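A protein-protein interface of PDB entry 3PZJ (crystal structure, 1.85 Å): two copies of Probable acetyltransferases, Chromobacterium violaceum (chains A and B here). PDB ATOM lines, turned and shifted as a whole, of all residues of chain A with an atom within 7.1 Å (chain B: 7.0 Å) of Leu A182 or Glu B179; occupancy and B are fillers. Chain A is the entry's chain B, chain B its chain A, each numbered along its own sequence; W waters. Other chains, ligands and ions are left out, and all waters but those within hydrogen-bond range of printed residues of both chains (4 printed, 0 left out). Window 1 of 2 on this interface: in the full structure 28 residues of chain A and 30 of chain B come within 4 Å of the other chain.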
ATOM      1  N   GLU A 157     -32.363  32.989   7.108  1.00  0.00           N
ATOM      2  CA  GLU A 157     -31.390  32.347   7.955  1.00  0.00           C
ATOM      3  C   GLU A 157     -30.403  33.351   8.428  1.00  0.00           C
ATOM      4  O   GLU A 157     -30.142  34.353   7.759  1.00  0.00           O
ATOM      5  CB  GLU A 157     -30.633  31.323   7.119  1.00  0.00           C
ATOM      6  CG  GLU A 157     -30.419  30.052   7.694  1.00  0.00           C
ATOM      7  CD  GLU A 157     -29.825  29.067   6.689  1.00  0.00           C
ATOM      8  OE1 GLU A 157     -30.511  28.122   6.363  1.00  0.00           O
ATOM      9  OE2 GLU A 157     -28.705  29.274   6.215  1.00  0.00           O
ATOM     10  N   ARG A 159     -26.450  32.827  10.264  1.00  0.00           N
ATOM     11  CA  ARG A 159     -25.442  31.824  10.641  1.00  0.00           C
ATOM     12  C   ARG A 159     -24.307  32.483  11.304  1.00  0.00           C
ATOM     13  O   ARG A 159     -23.970  33.624  10.977  1.00  0.00           O
ATOM     14  CB  ARG A 159     -24.892  31.084   9.469  1.00  0.00           C
ATOM     15  CG  ARG A 159     -25.872  30.298   8.708  1.00  0.00           C
ATOM     16  CD  ARG A 159     -25.161  29.500   7.488  1.00  0.00           C
ATOM     17  NE  ARG A 159     -26.134  28.585   6.926  1.00  0.00           N
ATOM     18  CZ  ARG A 159     -25.900  27.386   6.401  1.00  0.00           C
ATOM     19  NH1 ARG A 159     -26.912  26.684   5.956  1.00  0.00           N
ATOM     20  NH2 ARG A 159     -24.710  26.930   6.256  1.00  0.00           N
ATOM     21  N   PHE A 178     -33.006  29.244  17.138  1.00  0.00           N
ATOM     22  CA  PHE A 178     -31.820  28.372  16.916  1.00  0.00           C
ATOM     23  C   PHE A 178     -32.283  27.023  16.382  1.00  0.00           C
ATOM     24  O   PHE A 178     -33.203  26.436  16.918  1.00  0.00           O
ATOM     25  CB  PHE A 178     -30.938  28.233  18.172  1.00  0.00           C
ATOM     26  CG  PHE A 178     -29.871  27.197  18.059  1.00  0.00           C
ATOM     27  CD1 PHE A 178     -28.710  27.422  17.340  1.00  0.00           C
ATOM     28  CD2 PHE A 178     -30.012  25.960  18.710  1.00  0.00           C
ATOM     29  CE1 PHE A 178     -27.757  26.462  17.244  1.00  0.00           C
ATOM     30  CE2 PHE A 178     -29.007  24.978  18.617  1.00  0.00           C
ATOM     31  CZ  PHE A 178     -27.889  25.234  17.876  1.00  0.00           C
ATOM     32  N   GLU A 179     -31.732  26.579  15.252  1.00  0.00           N
ATOM     33  CA  GLU A 179     -32.118  25.286  14.673  1.00  0.00           C
ATOM     34  C   GLU A 179     -31.106  24.194  14.908  1.00  0.00           C
ATOM     35  O   GLU A 179     -31.460  23.028  15.031  1.00  0.00           O
ATOM     36  CB  GLU A 179     -32.338  25.436  13.157  1.00  0.00           C
ATOM     37  CG  GLU A 179     -33.666  26.162  12.844  1.00  0.00           C
ATOM     38  CD  GLU A 179     -33.948  26.293  11.360  1.00  0.00           C
ATOM     39  OE1 GLU A 179     -32.971  26.308  10.528  1.00  0.00           O
ATOM     40  OE2 GLU A 179     -35.158  26.465  11.021  1.00  0.00           O
ATOM     41  N   GLY A 180     -29.827  24.534  14.929  1.00  0.00           N
ATOM     42  CA  GLY A 180     -28.844  23.489  15.240  1.00  0.00           C
ATOM     43  C   GLY A 180     -27.444  23.933  14.817  1.00  0.00           C
ATOM     44  O   GLY A 180     -27.271  25.045  14.308  1.00  0.00           O
ATOM     45  N   THR A 181     -26.473  23.065  15.047  1.00  0.00           N
ATOM     46  CA  THR A 181     -25.063  23.393  14.845  1.00  0.00           C
ATOM     47  C   THR A 181     -24.463  22.422  13.835  1.00  0.00           C
ATOM     48  O   THR A 181     -24.534  21.189  14.012  1.00  0.00           O
ATOM     49  CB  THR A 181     -24.258  23.408  16.133  1.00  0.00           C
ATOM     50  OG1 THR A 181     -24.748  24.457  16.948  1.00  0.00           O
ATOM     51  CG2 THR A 181     -22.760  23.705  15.761  1.00  0.00           C
ATOM     52  N   LEU A 182     -23.991  22.994  12.724  1.00  0.00           N
ATOM     53  CA  LEU A 182     -23.297  22.263  11.710  1.00  0.00           C
ATOM     54  C   LEU A 182     -21.845  22.069  12.162  1.00  0.00           C
ATOM     55  O   LEU A 182     -21.007  22.999  12.086  1.00  0.00           O
ATOM     56  CB  LEU A 182     -23.365  23.040  10.352  1.00  0.00           C
ATOM     57  CG  LEU A 182     -24.719  23.502   9.785  1.00  0.00           C
ATOM     58  CD1 LEU A 182     -24.701  24.314   8.399  1.00  0.00           C
ATOM     59  CD2 LEU A 182     -25.704  22.292   9.642  1.00  0.00           C
ATOM     60  N   ARG A 183     -21.544  20.885  12.631  1.00  0.00           N
ATOM     61  CA  ARG A 183     -20.255  20.567  13.207  1.00  0.00           C
ATOM     62  C   ARG A 183     -19.139  20.453  12.203  1.00  0.00           C
ATOM     63  O   ARG A 183     -19.289  19.843  11.151  1.00  0.00           O
ATOM     64  CB  ARG A 183     -20.365  19.309  14.059  1.00  0.00           C
ATOM     65  CG  ARG A 183     -21.482  19.287  15.066  1.00  0.00           C
ATOM     66  CD  ARG A 183     -21.657  17.857  15.572  1.00  0.00           C
ATOM     67  NE  ARG A 183     -21.906  16.823  14.556  1.00  0.00           N
ATOM     68  CZ  ARG A 183     -21.566  15.521  14.692  1.00  0.00           C
ATOM     69  NH1 ARG A 183     -20.990  15.032  15.804  1.00  0.00           N
ATOM     70  NH2 ARG A 183     -21.825  14.686  13.732  1.00  0.00           N
ATOM     71  N   GLN A 184     -17.983  21.066  12.485  1.00  0.00           N
ATOM     72  CA  GLN A 184     -16.895  21.001  11.475  1.00  0.00           C
ATOM     73  C   GLN A 184     -17.326  21.438  10.079  1.00  0.00           C
ATOM     74  O   GLN A 184     -16.933  20.849   9.085  1.00  0.00           O
ATOM     75  CB  GLN A 184     -16.219  19.580  11.406  1.00  0.00           C
ATOM     76  CG  GLN A 184     -15.621  19.145  12.749  1.00  0.00           C
ATOM     77  CD  GLN A 184     -14.771  17.933  12.798  1.00  0.00           C
ATOM     78  OE1 GLN A 184     -14.268  17.601  13.879  1.00  0.00           O
ATOM     79  NE2 GLN A 184     -14.546  17.250  11.666  1.00  0.00           N
ATOM     80  N   ALA A 185     -18.116  22.501  10.017  1.00  0.00           N
ATOM     81  CA  ALA A 185     -18.622  23.001   8.774  1.00  0.00           C
ATOM     82  C   ALA A 185     -17.548  23.645   7.904  1.00  0.00           C
ATOM     83  O   ALA A 185     -17.624  23.585   6.682  1.00  0.00           O
ATOM     84  CB  ALA A 185     -19.722  24.018   9.051  1.00  0.00           C
ATOM     85  N   MET A 186     -16.592  24.339   8.523  1.00  0.00           N
ATOM     86  CA  MET A 186     -15.557  25.100   7.807  1.00  0.00           C
ATOM     87  C   MET A 186     -14.205  25.049   8.557  1.00  0.00           C
ATOM     88  O   MET A 186     -14.148  24.669   9.713  1.00  0.00           O
ATOM     89  CB  MET A 186     -16.032  26.565   7.688  1.00  0.00           C
ATOM     90  CG  MET A 186     -17.273  26.687   6.794  1.00  0.00           C
ATOM     91  SD  MET A 186     -17.842  28.595   6.904  1.00  0.00           S
ATOM     92  CE  MET A 186     -16.427  29.241   6.033  1.00  0.00           C
ATOM     93  N   ASN A 192     -10.844  25.049  13.415  1.00  0.00           N
ATOM     94  CA  ASN A 192     -12.187  24.536  13.251  1.00  0.00           C
ATOM     95  C   ASN A 192     -13.285  25.610  13.369  1.00  0.00           C
ATOM     96  O   ASN A 192     -13.234  26.453  14.263  1.00  0.00           O
ATOM     97  CB  ASN A 192     -12.509  23.486  14.297  1.00  0.00           C
ATOM     98  CG  ASN A 192     -13.907  22.850  14.052  1.00  0.00           C
ATOM     99  OD1 ASN A 192     -14.153  22.225  13.023  1.00  0.00           O
ATOM    100  ND2 ASN A 192     -14.815  23.089  14.946  1.00  0.00           N
ATOM    101  N   ARG A 193     -14.313  25.496  12.550  1.00  0.00           N
ATOM    102  CA  ARG A 193     -15.517  26.258  12.748  1.00  0.00           C
ATOM    103  C   ARG A 193     -16.776  25.378  12.778  1.00  0.00           C
ATOM    104  O   ARG A 193     -17.045  24.688  11.860  1.00  0.00           O
ATOM    105  CB  ARG A 193     -15.714  27.320  11.654  1.00  0.00           C
ATOM    106  CG  ARG A 193     -17.143  27.845  11.633  1.00  0.00           C
ATOM    107  CD  ARG A 193     -17.337  29.091  10.838  1.00  0.00           C
ATOM    108  NE  ARG A 193     -18.720  29.334  10.539  1.00  0.00           N
ATOM    109  CZ  ARG A 193     -19.231  30.463  10.098  1.00  0.00           C
ATOM    110  NH1 ARG A 193     -20.513  30.533   9.856  1.00  0.00           N
ATOM    111  NH2 ARG A 193     -18.476  31.511   9.888  1.00  0.00           N
ATOM    112  N   ASP A 194     -17.509  25.434  13.859  1.00  0.00           N
ATOM    113  CA  ASP A 194     -18.870  24.934  13.884  1.00  0.00           C
ATOM    114  C   ASP A 194     -19.819  26.094  13.619  1.00  0.00           C
ATOM    115  O   ASP A 194     -19.654  27.181  14.167  1.00  0.00           O
ATOM    116  CB  ASP A 194     -19.217  24.297  15.236  1.00  0.00           C
ATOM    117  CG  ASP A 194     -18.293  23.104  15.630  1.00  0.00           C
ATOM    118  OD1 ASP A 194     -17.647  22.440  14.811  1.00  0.00           O
ATOM    119  OD2 ASP A 194     -18.217  22.889  16.860  1.00  0.00           O
ATOM    120  N   THR A 195     -20.829  25.907  12.762  1.00  0.00           N
ATOM    121  CA  THR A 195     -21.708  27.007  12.401  1.00  0.00           C
ATOM    122  C   THR A 195     -23.014  26.850  13.143  1.00  0.00           C
ATOM    123  O   THR A 195     -23.727  25.873  12.923  1.00  0.00           O
ATOM    124  CB  THR A 195     -21.939  27.037  10.885  1.00  0.00           C
ATOM    125  OG1 THR A 195     -20.702  27.326  10.240  1.00  0.00           O
ATOM    126  CG2 THR A 195     -23.001  28.008  10.452  1.00  0.00           C
ATOM    127  N   HIS A 196     -23.380  27.848  13.954  1.00  0.00           N
ATOM    128  CA  HIS A 196     -24.738  27.868  14.495  1.00  0.00           C
ATOM    129  C   HIS A 196     -25.690  28.355  13.364  1.00  0.00           C
ATOM    130  O   HIS A 196     -25.393  29.350  12.710  1.00  0.00           O
ATOM    131  CB  HIS A 196     -24.856  28.805  15.664  1.00  0.00           C
ATOM    132  CG  HIS A 196     -24.192  28.313  16.903  1.00  0.00           C
ATOM    133  ND1 HIS A 196     -24.101  26.961  17.219  1.00  0.00           N
ATOM    134  CD2 HIS A 196     -23.702  28.998  17.966  1.00  0.00           C
ATOM    135  CE1 HIS A 196     -23.473  26.859  18.382  1.00  0.00           C
ATOM    136  NE2 HIS A 196     -23.266  28.082  18.869  1.00  0.00           N
ATOM    137  N   VAL A 197     -26.803  27.667  13.185  1.00  0.00           N
ATOM    138  CA  VAL A 197     -27.827  28.068  12.192  1.00  0.00           C
ATOM    139  C   VAL A 197     -29.121  28.500  12.904  1.00  0.00           C
ATOM    140  O   VAL A 197     -29.705  27.741  13.722  1.00  0.00           O
ATOM    141  CB  VAL A 197     -28.112  26.911  11.229  1.00  0.00           C
ATOM    142  CG1 VAL A 197     -29.312  27.290  10.255  1.00  0.00           C
ATOM    143  CG2 VAL A 197     -26.807  26.428  10.475  1.00  0.00           C
ATOM    144  N   ARG B 155     -16.278  16.562   7.154  1.00  0.00           N
ATOM    145  CA  ARG B 155     -17.684  16.533   7.473  1.00  0.00           C
ATOM    146  C   ARG B 155     -18.437  15.965   6.236  1.00  0.00           C
ATOM    147  O   ARG B 155     -18.249  16.492   5.124  1.00  0.00           O
ATOM    148  CB  ARG B 155     -18.143  17.986   7.704  1.00  0.00           C
ATOM    149  CG  ARG B 155     -19.659  18.158   7.911  1.00  0.00           C
ATOM    150  CD  ARG B 155     -20.096  19.618   7.826  1.00  0.00           C
ATOM    151  NE  ARG B 155     -21.538  19.768   7.847  1.00  0.00           N
ATOM    152  CZ  ARG B 155     -22.348  19.451   8.897  1.00  0.00           C
ATOM    153  NH1 ARG B 155     -21.891  19.089  10.079  1.00  0.00           N
ATOM    154  NH2 ARG B 155     -23.641  19.508   8.743  1.00  0.00           N
ATOM    155  N   GLU B 157     -22.424  15.241   5.060  1.00  0.00           N
ATOM    156  CA  GLU B 157     -23.790  15.437   5.460  1.00  0.00           C
ATOM    157  C   GLU B 157     -24.671  14.392   4.820  1.00  0.00           C
ATOM    158  O   GLU B 157     -24.336  13.832   3.814  1.00  0.00           O
ATOM    159  CB  GLU B 157     -24.306  16.791   5.011  1.00  0.00           C
ATOM    160  CG  GLU B 157     -23.862  17.869   5.809  1.00  0.00           C
ATOM    161  CD  GLU B 157     -24.450  19.193   5.409  1.00  0.00           C
ATOM    162  OE1 GLU B 157     -24.160  20.122   6.103  1.00  0.00           O
ATOM    163  OE2 GLU B 157     -25.165  19.288   4.441  1.00  0.00           O
ATOM    164  N   ARG B 159     -28.886  14.714   4.145  1.00  0.00           N
ATOM    165  CA  ARG B 159     -30.077  15.579   4.290  1.00  0.00           C
ATOM    166  C   ARG B 159     -31.345  14.901   3.712  1.00  0.00           C
ATOM    167  O   ARG B 159     -31.294  14.153   2.736  1.00  0.00           O
ATOM    168  CB  ARG B 159     -29.930  16.883   3.536  1.00  0.00           C
ATOM    169  CG  ARG B 159     -28.913  17.786   4.075  1.00  0.00           C
ATOM    170  CD  ARG B 159     -28.848  19.155   3.360  1.00  0.00           C
ATOM    171  NE  ARG B 159     -27.819  19.948   4.014  1.00  0.00           N
ATOM    172  CZ  ARG B 159     -27.872  21.258   4.193  1.00  0.00           C
ATOM    173  NH1 ARG B 159     -26.848  21.882   4.752  1.00  0.00           N
ATOM    174  NH2 ARG B 159     -28.901  21.917   3.737  1.00  0.00           N
ATOM    175  N   ARG B 172     -29.466   7.499  10.417  1.00  0.00           N
ATOM    176  CA  ARG B 172     -29.116   7.085  11.783  1.00  0.00           C
ATOM    177  C   ARG B 172     -28.515   5.676  11.822  1.00  0.00           C
ATOM    178  O   ARG B 172     -27.573   5.432  12.570  1.00  0.00           O
ATOM    179  CB  ARG B 172     -30.336   7.238  12.723  1.00  0.00           C
ATOM    180  CG  ARG B 172     -30.642   8.650  13.079  1.00  0.00           C
ATOM    181  CD  ARG B 172     -31.994   8.766  13.806  1.00  0.00           C
ATOM    182  NE  ARG B 172     -32.449  10.089  14.221  1.00  0.00           N
ATOM    183  CZ  ARG B 172     -31.916  10.815  15.208  1.00  0.00           C
ATOM    184  NH1 ARG B 172     -30.871  10.403  15.893  1.00  0.00           N
ATOM    185  NH2 ARG B 172     -32.464  11.952  15.538  1.00  0.00           N
ATOM    186  N   GLN B 177     -25.096  11.576  12.724  1.00  0.00           N
ATOM    187  CA  GLN B 177     -25.732  12.159  13.876  1.00  0.00           C
ATOM    188  C   GLN B 177     -26.703  13.222  13.437  1.00  0.00           C
ATOM    189  O   GLN B 177     -26.356  14.049  12.561  1.00  0.00           O
ATOM    190  CB  GLN B 177     -24.665  12.840  14.734  1.00  0.00           C
ATOM    191  CG  GLN B 177     -23.536  11.947  15.242  1.00  0.00           C
ATOM    192  CD  GLN B 177     -24.085  10.706  15.932  1.00  0.00           C
ATOM    193  OE1 GLN B 177     -23.849   9.556  15.494  1.00  0.00           O
ATOM    194  NE2 GLN B 177     -24.869  10.935  16.978  1.00  0.00           N
ATOM    195  N   PHE B 178     -27.835  13.310  14.126  1.00  0.00           N
ATOM    196  CA  PHE B 178     -28.824  14.349  13.822  1.00  0.00           C
ATOM    197  C   PHE B 178     -28.362  15.657  14.352  1.00  0.00           C
ATOM    198  O   PHE B 178     -27.968  15.722  15.536  1.00  0.00           O
ATOM    199  CB  PHE B 178     -30.201  13.989  14.451  1.00  0.00           C
ATOM    200  CG  PHE B 178     -31.236  15.011  14.225  1.00  0.00           C
ATOM    201  CD1 PHE B 178     -31.644  15.322  12.958  1.00  0.00           C
ATOM    202  CD2 PHE B 178     -31.732  15.747  15.290  1.00  0.00           C
ATOM    203  CE1 PHE B 178     -32.630  16.377  12.750  1.00  0.00           C
ATOM    204  CE2 PHE B 178     -32.693  16.779  15.097  1.00  0.00           C
ATOM    205  CZ  PHE B 178     -33.137  17.064  13.810  1.00  0.00           C
ATOM    206  N   GLU B 179     -28.378  16.715  13.509  1.00  0.00           N
ATOM    207  CA  GLU B 179     -27.945  18.020  13.941  1.00  0.00           C
ATOM    208  C   GLU B 179     -29.110  19.020  14.137  1.00  0.00           C
ATOM    209  O   GLU B 179     -29.070  19.856  15.031  1.00  0.00           O
ATOM    210  CB  GLU B 179     -26.923  18.619  12.952  1.00  0.00           C
ATOM    211  CG  GLU B 179     -25.574  17.947  13.056  1.00  0.00           C
ATOM    212  CD  GLU B 179     -24.550  18.522  12.137  1.00  0.00           C
ATOM    213  OE1 GLU B 179     -24.891  19.032  11.050  1.00  0.00           O
ATOM    214  OE2 GLU B 179     -23.363  18.341  12.458  1.00  0.00           O
ATOM    215  N   GLY B 180     -30.089  18.966  13.281  1.00  0.00           N
ATOM    216  CA  GLY B 180     -31.249  19.813  13.410  1.00  0.00           C
ATOM    217  C   GLY B 180     -32.049  19.832  12.124  1.00  0.00           C
ATOM    218  O   GLY B 180     -31.695  19.119  11.162  1.00  0.00           O
ATOM    219  N   THR B 181     -33.111  20.621  12.135  1.00  0.00           N
ATOM    220  CA  THR B 181     -34.034  20.734  11.059  1.00  0.00           C
ATOM    221  C   THR B 181     -34.176  22.177  10.592  1.00  0.00           C
ATOM    222  O   THR B 181     -34.448  23.052  11.343  1.00  0.00           O
ATOM    223  CB  THR B 181     -35.420  20.228  11.460  1.00  0.00           C
ATOM    224  OG1 THR B 181     -35.354  18.886  11.915  1.00  0.00           O
ATOM    225  CG2 THR B 181     -36.384  20.346  10.297  1.00  0.00           C
ATOM    226  N   LEU B 182     -33.957  22.346   9.302  1.00  0.00           N
ATOM    227  CA  LEU B 182     -34.085  23.597   8.607  1.00  0.00           C
ATOM    228  C   LEU B 182     -35.561  23.757   8.180  1.00  0.00           C
ATOM    229  O   LEU B 182     -36.026  23.147   7.194  1.00  0.00           O
ATOM    230  CB  LEU B 182     -33.140  23.635   7.418  1.00  0.00           C
ATOM    231  CG  LEU B 182     -31.692  24.058   7.611  1.00  0.00           C
ATOM    232  CD1 LEU B 182     -31.156  23.787   9.016  1.00  0.00           C
ATOM    233  CD2 LEU B 182     -30.790  23.514   6.473  1.00  0.00           C
ATOM    234  N   HIS B 196     -34.198  17.820   7.395  1.00  0.00           N
ATOM    235  CA  HIS B 196     -33.354  17.315   8.463  1.00  0.00           C
ATOM    236  C   HIS B 196     -31.903  17.261   7.986  1.00  0.00           C
ATOM    237  O   HIS B 196     -31.633  16.757   6.842  1.00  0.00           O
ATOM    238  CB  HIS B 196     -33.744  15.867   8.838  1.00  0.00           C
ATOM    239  CG  HIS B 196     -35.079  15.696   9.520  1.00  0.00           C
ATOM    240  ND1 HIS B 196     -35.654  16.636  10.346  1.00  0.00           N
ATOM    241  CD2 HIS B 196     -35.909  14.610   9.546  1.00  0.00           C
ATOM    242  CE1 HIS B 196     -36.793  16.145  10.837  1.00  0.00           C
ATOM    243  NE2 HIS B 196     -36.975  14.930  10.350  1.00  0.00           N
ATOM    244  N   VAL B 197     -30.976  17.716   8.840  1.00  0.00           N
ATOM    245  CA  VAL B 197     -29.540  17.640   8.560  1.00  0.00           C
ATOM    246  C   VAL B 197     -28.872  16.716   9.541  1.00  0.00           C
ATOM    247  O   VAL B 197     -29.051  16.840  10.785  1.00  0.00           O
ATOM    248  CB  VAL B 197     -28.856  19.032   8.600  1.00  0.00           C
ATOM    249  CG1 VAL B 197     -27.331  18.901   8.283  1.00  0.00           C
ATOM    250  CG2 VAL B 197     -29.538  20.005   7.631  1.00  0.00           C
ATOM    251  N   PHE B 198     -28.149  15.743   8.987  1.00  0.00           N
ATOM    252  CA  PHE B 198     -27.375  14.797   9.707  1.00  0.00           C
ATOM    253  C   PHE B 198     -25.908  14.920   9.255  1.00  0.00           C
ATOM    254  O   PHE B 198     -25.672  15.320   8.146  1.00  0.00           O
ATOM    255  CB  PHE B 198     -27.796  13.379   9.393  1.00  0.00           C
ATOM    256  CG  PHE B 198     -29.230  13.064   9.692  1.00  0.00           C
ATOM    257  CD1 PHE B 198     -29.583  12.412  10.877  1.00  0.00           C
ATOM    258  CD2 PHE B 198     -30.227  13.309   8.756  1.00  0.00           C
ATOM    259  CE1 PHE B 198     -30.921  12.084  11.133  1.00  0.00           C
ATOM    260  CE2 PHE B 198     -31.534  12.984   9.021  1.00  0.00           C
ATOM    261  CZ  PHE B 198     -31.887  12.414  10.229  1.00  0.00           C
ATOM    262  N   SER B 199     -24.951  14.477  10.065  1.00  0.00           N
ATOM    263  CA  SER B 199     -23.563  14.511   9.675  1.00  0.00           C
ATOM    264  C   SER B 199     -22.724  13.455  10.312  1.00  0.00           C
ATOM    265  O   SER B 199     -23.057  12.929  11.379  1.00  0.00           O
ATOM    266  CB  SER B 199     -22.928  15.881   9.964  1.00  0.00           C
ATOM    267  OG  SER B 199     -22.652  16.018  11.346  1.00  0.00           O
ATOM    268  N   MET B 200     -21.612  13.158   9.643  1.00  0.00           N
ATOM    269  CA  MET B 200     -20.584  12.252  10.133  1.00  0.00           C
ATOM    270  C   MET B 200     -19.222  12.928   9.978  1.00  0.00           C
ATOM    271  O   MET B 200     -18.809  13.276   8.872  1.00  0.00           O
ATOM    272  CB  MET B 200     -20.614  10.933   9.360  1.00  0.00           C
ATOM    273  CG  MET B 200     -19.240  10.338   9.095  1.00  0.00           C
ATOM    274  SD  MET B 200     -19.161   8.428   9.481  1.00  0.00           S
ATOM    275  CE  MET B 200     -19.828   8.461  11.312  1.00  0.00           C
ATOM    276  N   LEU B 201     -18.538  13.114  11.101  1.00  0.00           N
ATOM    277  CA  LEU B 201     -17.312  13.833  11.161  1.00  0.00           C
ATOM    278  C   LEU B 201     -16.170  12.870  10.965  1.00  0.00           C
ATOM    279  O   LEU B 201     -16.303  11.650  11.205  1.00  0.00           O
ATOM    280  CB  LEU B 201     -17.173  14.480  12.515  1.00  0.00           C
ATOM    281  CG  LEU B 201     -18.229  15.466  12.987  1.00  0.00           C
ATOM    282  CD1 LEU B 201     -17.732  16.229  14.194  1.00  0.00           C
ATOM    283  CD2 LEU B 201     -18.553  16.475  11.839  1.00  0.00           C
HETATM  284  O   HOH W   1     -33.898  21.721  14.765  1.00  0.00           O
HETATM  285  O   HOH W   2     -27.145  20.811  16.654  1.00  0.00           O
HETATM  286  O   HOH W   3     -28.444  24.631   3.814  1.00  0.00           O
HETATM  287  O   HOH W   4     -25.058  24.482   4.741  1.00  0.00           O
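Glu B179 touches its own counterpart, Glu A179.
Glu A179 touches Gly B180, and with the chains exchanged Gly A180 touches Glu B179.
Glu A179 touches Leu B182, and with the chains exchanged Leu A182 touches Glu B179.
Leu A182 touches Val B197, but with the chains exchanged Val A197 does not touch Leu B182 (4.1 Å).
Positions printed for both chains: 157, 159, 178, 179, 180, 181, 182, 196 and 197.
The backbone NH (N) of Val B197 sits at hydrogen-bond distance from the backbone carbonyl oxygen (O) of Gly B180, at 2.8 Å.
The side-chain hydroxyl (OG) of Ser B199 sits at hydrogen-bond distance from the side-chain carboxylate (OE2) of Glu B179, at 2.7 Å.
The backbone carbonyl oxygen of Ser B199 sits at hydrogen-bond distance from the backbone NH of Gln B177 (2.8 Å).
The side-chain hydroxyl (OG1) of Thr A181 sits at hydrogen-bond distance from a ring nitrogen (ND1) of His A196 (2.6 Å).
The side-chain hydroxyl (OG1) of Thr B181 lies within hydrogen-bond range of a ring nitrogen (ND1) of His B196 (2.8 Å).
The backbone carbonyl oxygen (O) of Thr A195 is in hydrogen-bond range of the backbone NH (N) of Leu A182 (2.9 Å).
Of the 16 printed residues of chain B, 9 touch a printed residue of chain A.
Hydrophobic or aromatic side chains of chain B within 4 Å of the printed part of chain A: Leu B182, Val B197 and Leu B201.
Hydrophobic or aromatic side chains of chain A that line the printed part of chain B: Leu A182.
Among the printed residues, Asp or Glu carboxylates within 4 Å of a Lys or Arg side-chain nitrogen of the other chain: Arg A183 with Glu B179 (3.0 Å).
Of the printed residues of chain B, Leu A182 touches Arg B155 (3.6 Å), Glu B179 (3.6 Å) and Val B197 (3.999 Å).
Printed residues of chain A within 4 Å of Glu B179: Glu A179, Gly A180, Thr A181, Leu A182 and Arg A183.
Of the printed residues of chain A, Gln B177 touches Arg A183.
Of the printed residues of chain B, Thr A181 touches Glu B179.
The nearest printed residue of chain B that does not touch Leu A182 is Glu B157 (4.4 Å).
The nearest residue of chain A that does not touch Glu B179 is Gln A184 (6.0 Å).
Water W2 lies within hydrogen-bond range of O of Glu B179 (2.7 Å) and N of Thr A181 (2.8 Å).
Water W3 bridges NH2 of Arg B159 (2.8 Å) and NH1 of Arg A159 (3.3 Å).
Water W1 lies within hydrogen-bond range of O of Glu A179 (2.8 Å) and N of Thr B181 (3.0 Å).
Water W4 lies within hydrogen-bond range of NH2 of Arg A159 (2.9 Å) and NH1 of Arg B159 (3.2 Å).
Gly B180 touches Glu A179.
CD1 of Leu B182 touches OE1 of Glu A179 (3.5 Å).
Glu B179 touches Gly A180 (O to CA, 3.6 Å).
OE1 of Glu B179 touches CD2 of Leu A182, at 3.6 Å.
Val B197 touches Leu A182 (CG1 to CD2, 3.999 Å).
Arg A183 touches Gln B177.
O of Arg A183 touches CD2 of Leu B201, at 3.5 Å.
Gln A184 touches Arg B155 (O to CB, 3.4 Å).
Gln A184 touches Leu B201 (CD to CD1, 3.7 Å).
CA of Ala A185 touches CD of Arg B155, 3.8 Å away.
The backbone carbonyl oxygen (O) of Thr A181 sits close to the side-chain carboxylate (OE2) of Glu B179, at 3.4 Å.
The side-chain hydroxyl of Ser B199 sits at hydrogen-bond distance from the guanidinium group of Arg A183 (2.9 Å).
OE2 of Glu B179 is in salt-bridge range of NE of Arg A183 (3.0 Å).
NH1 of Arg B155 lies within hydrogen-bond range of O of Arg A183, at 2.9 Å.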
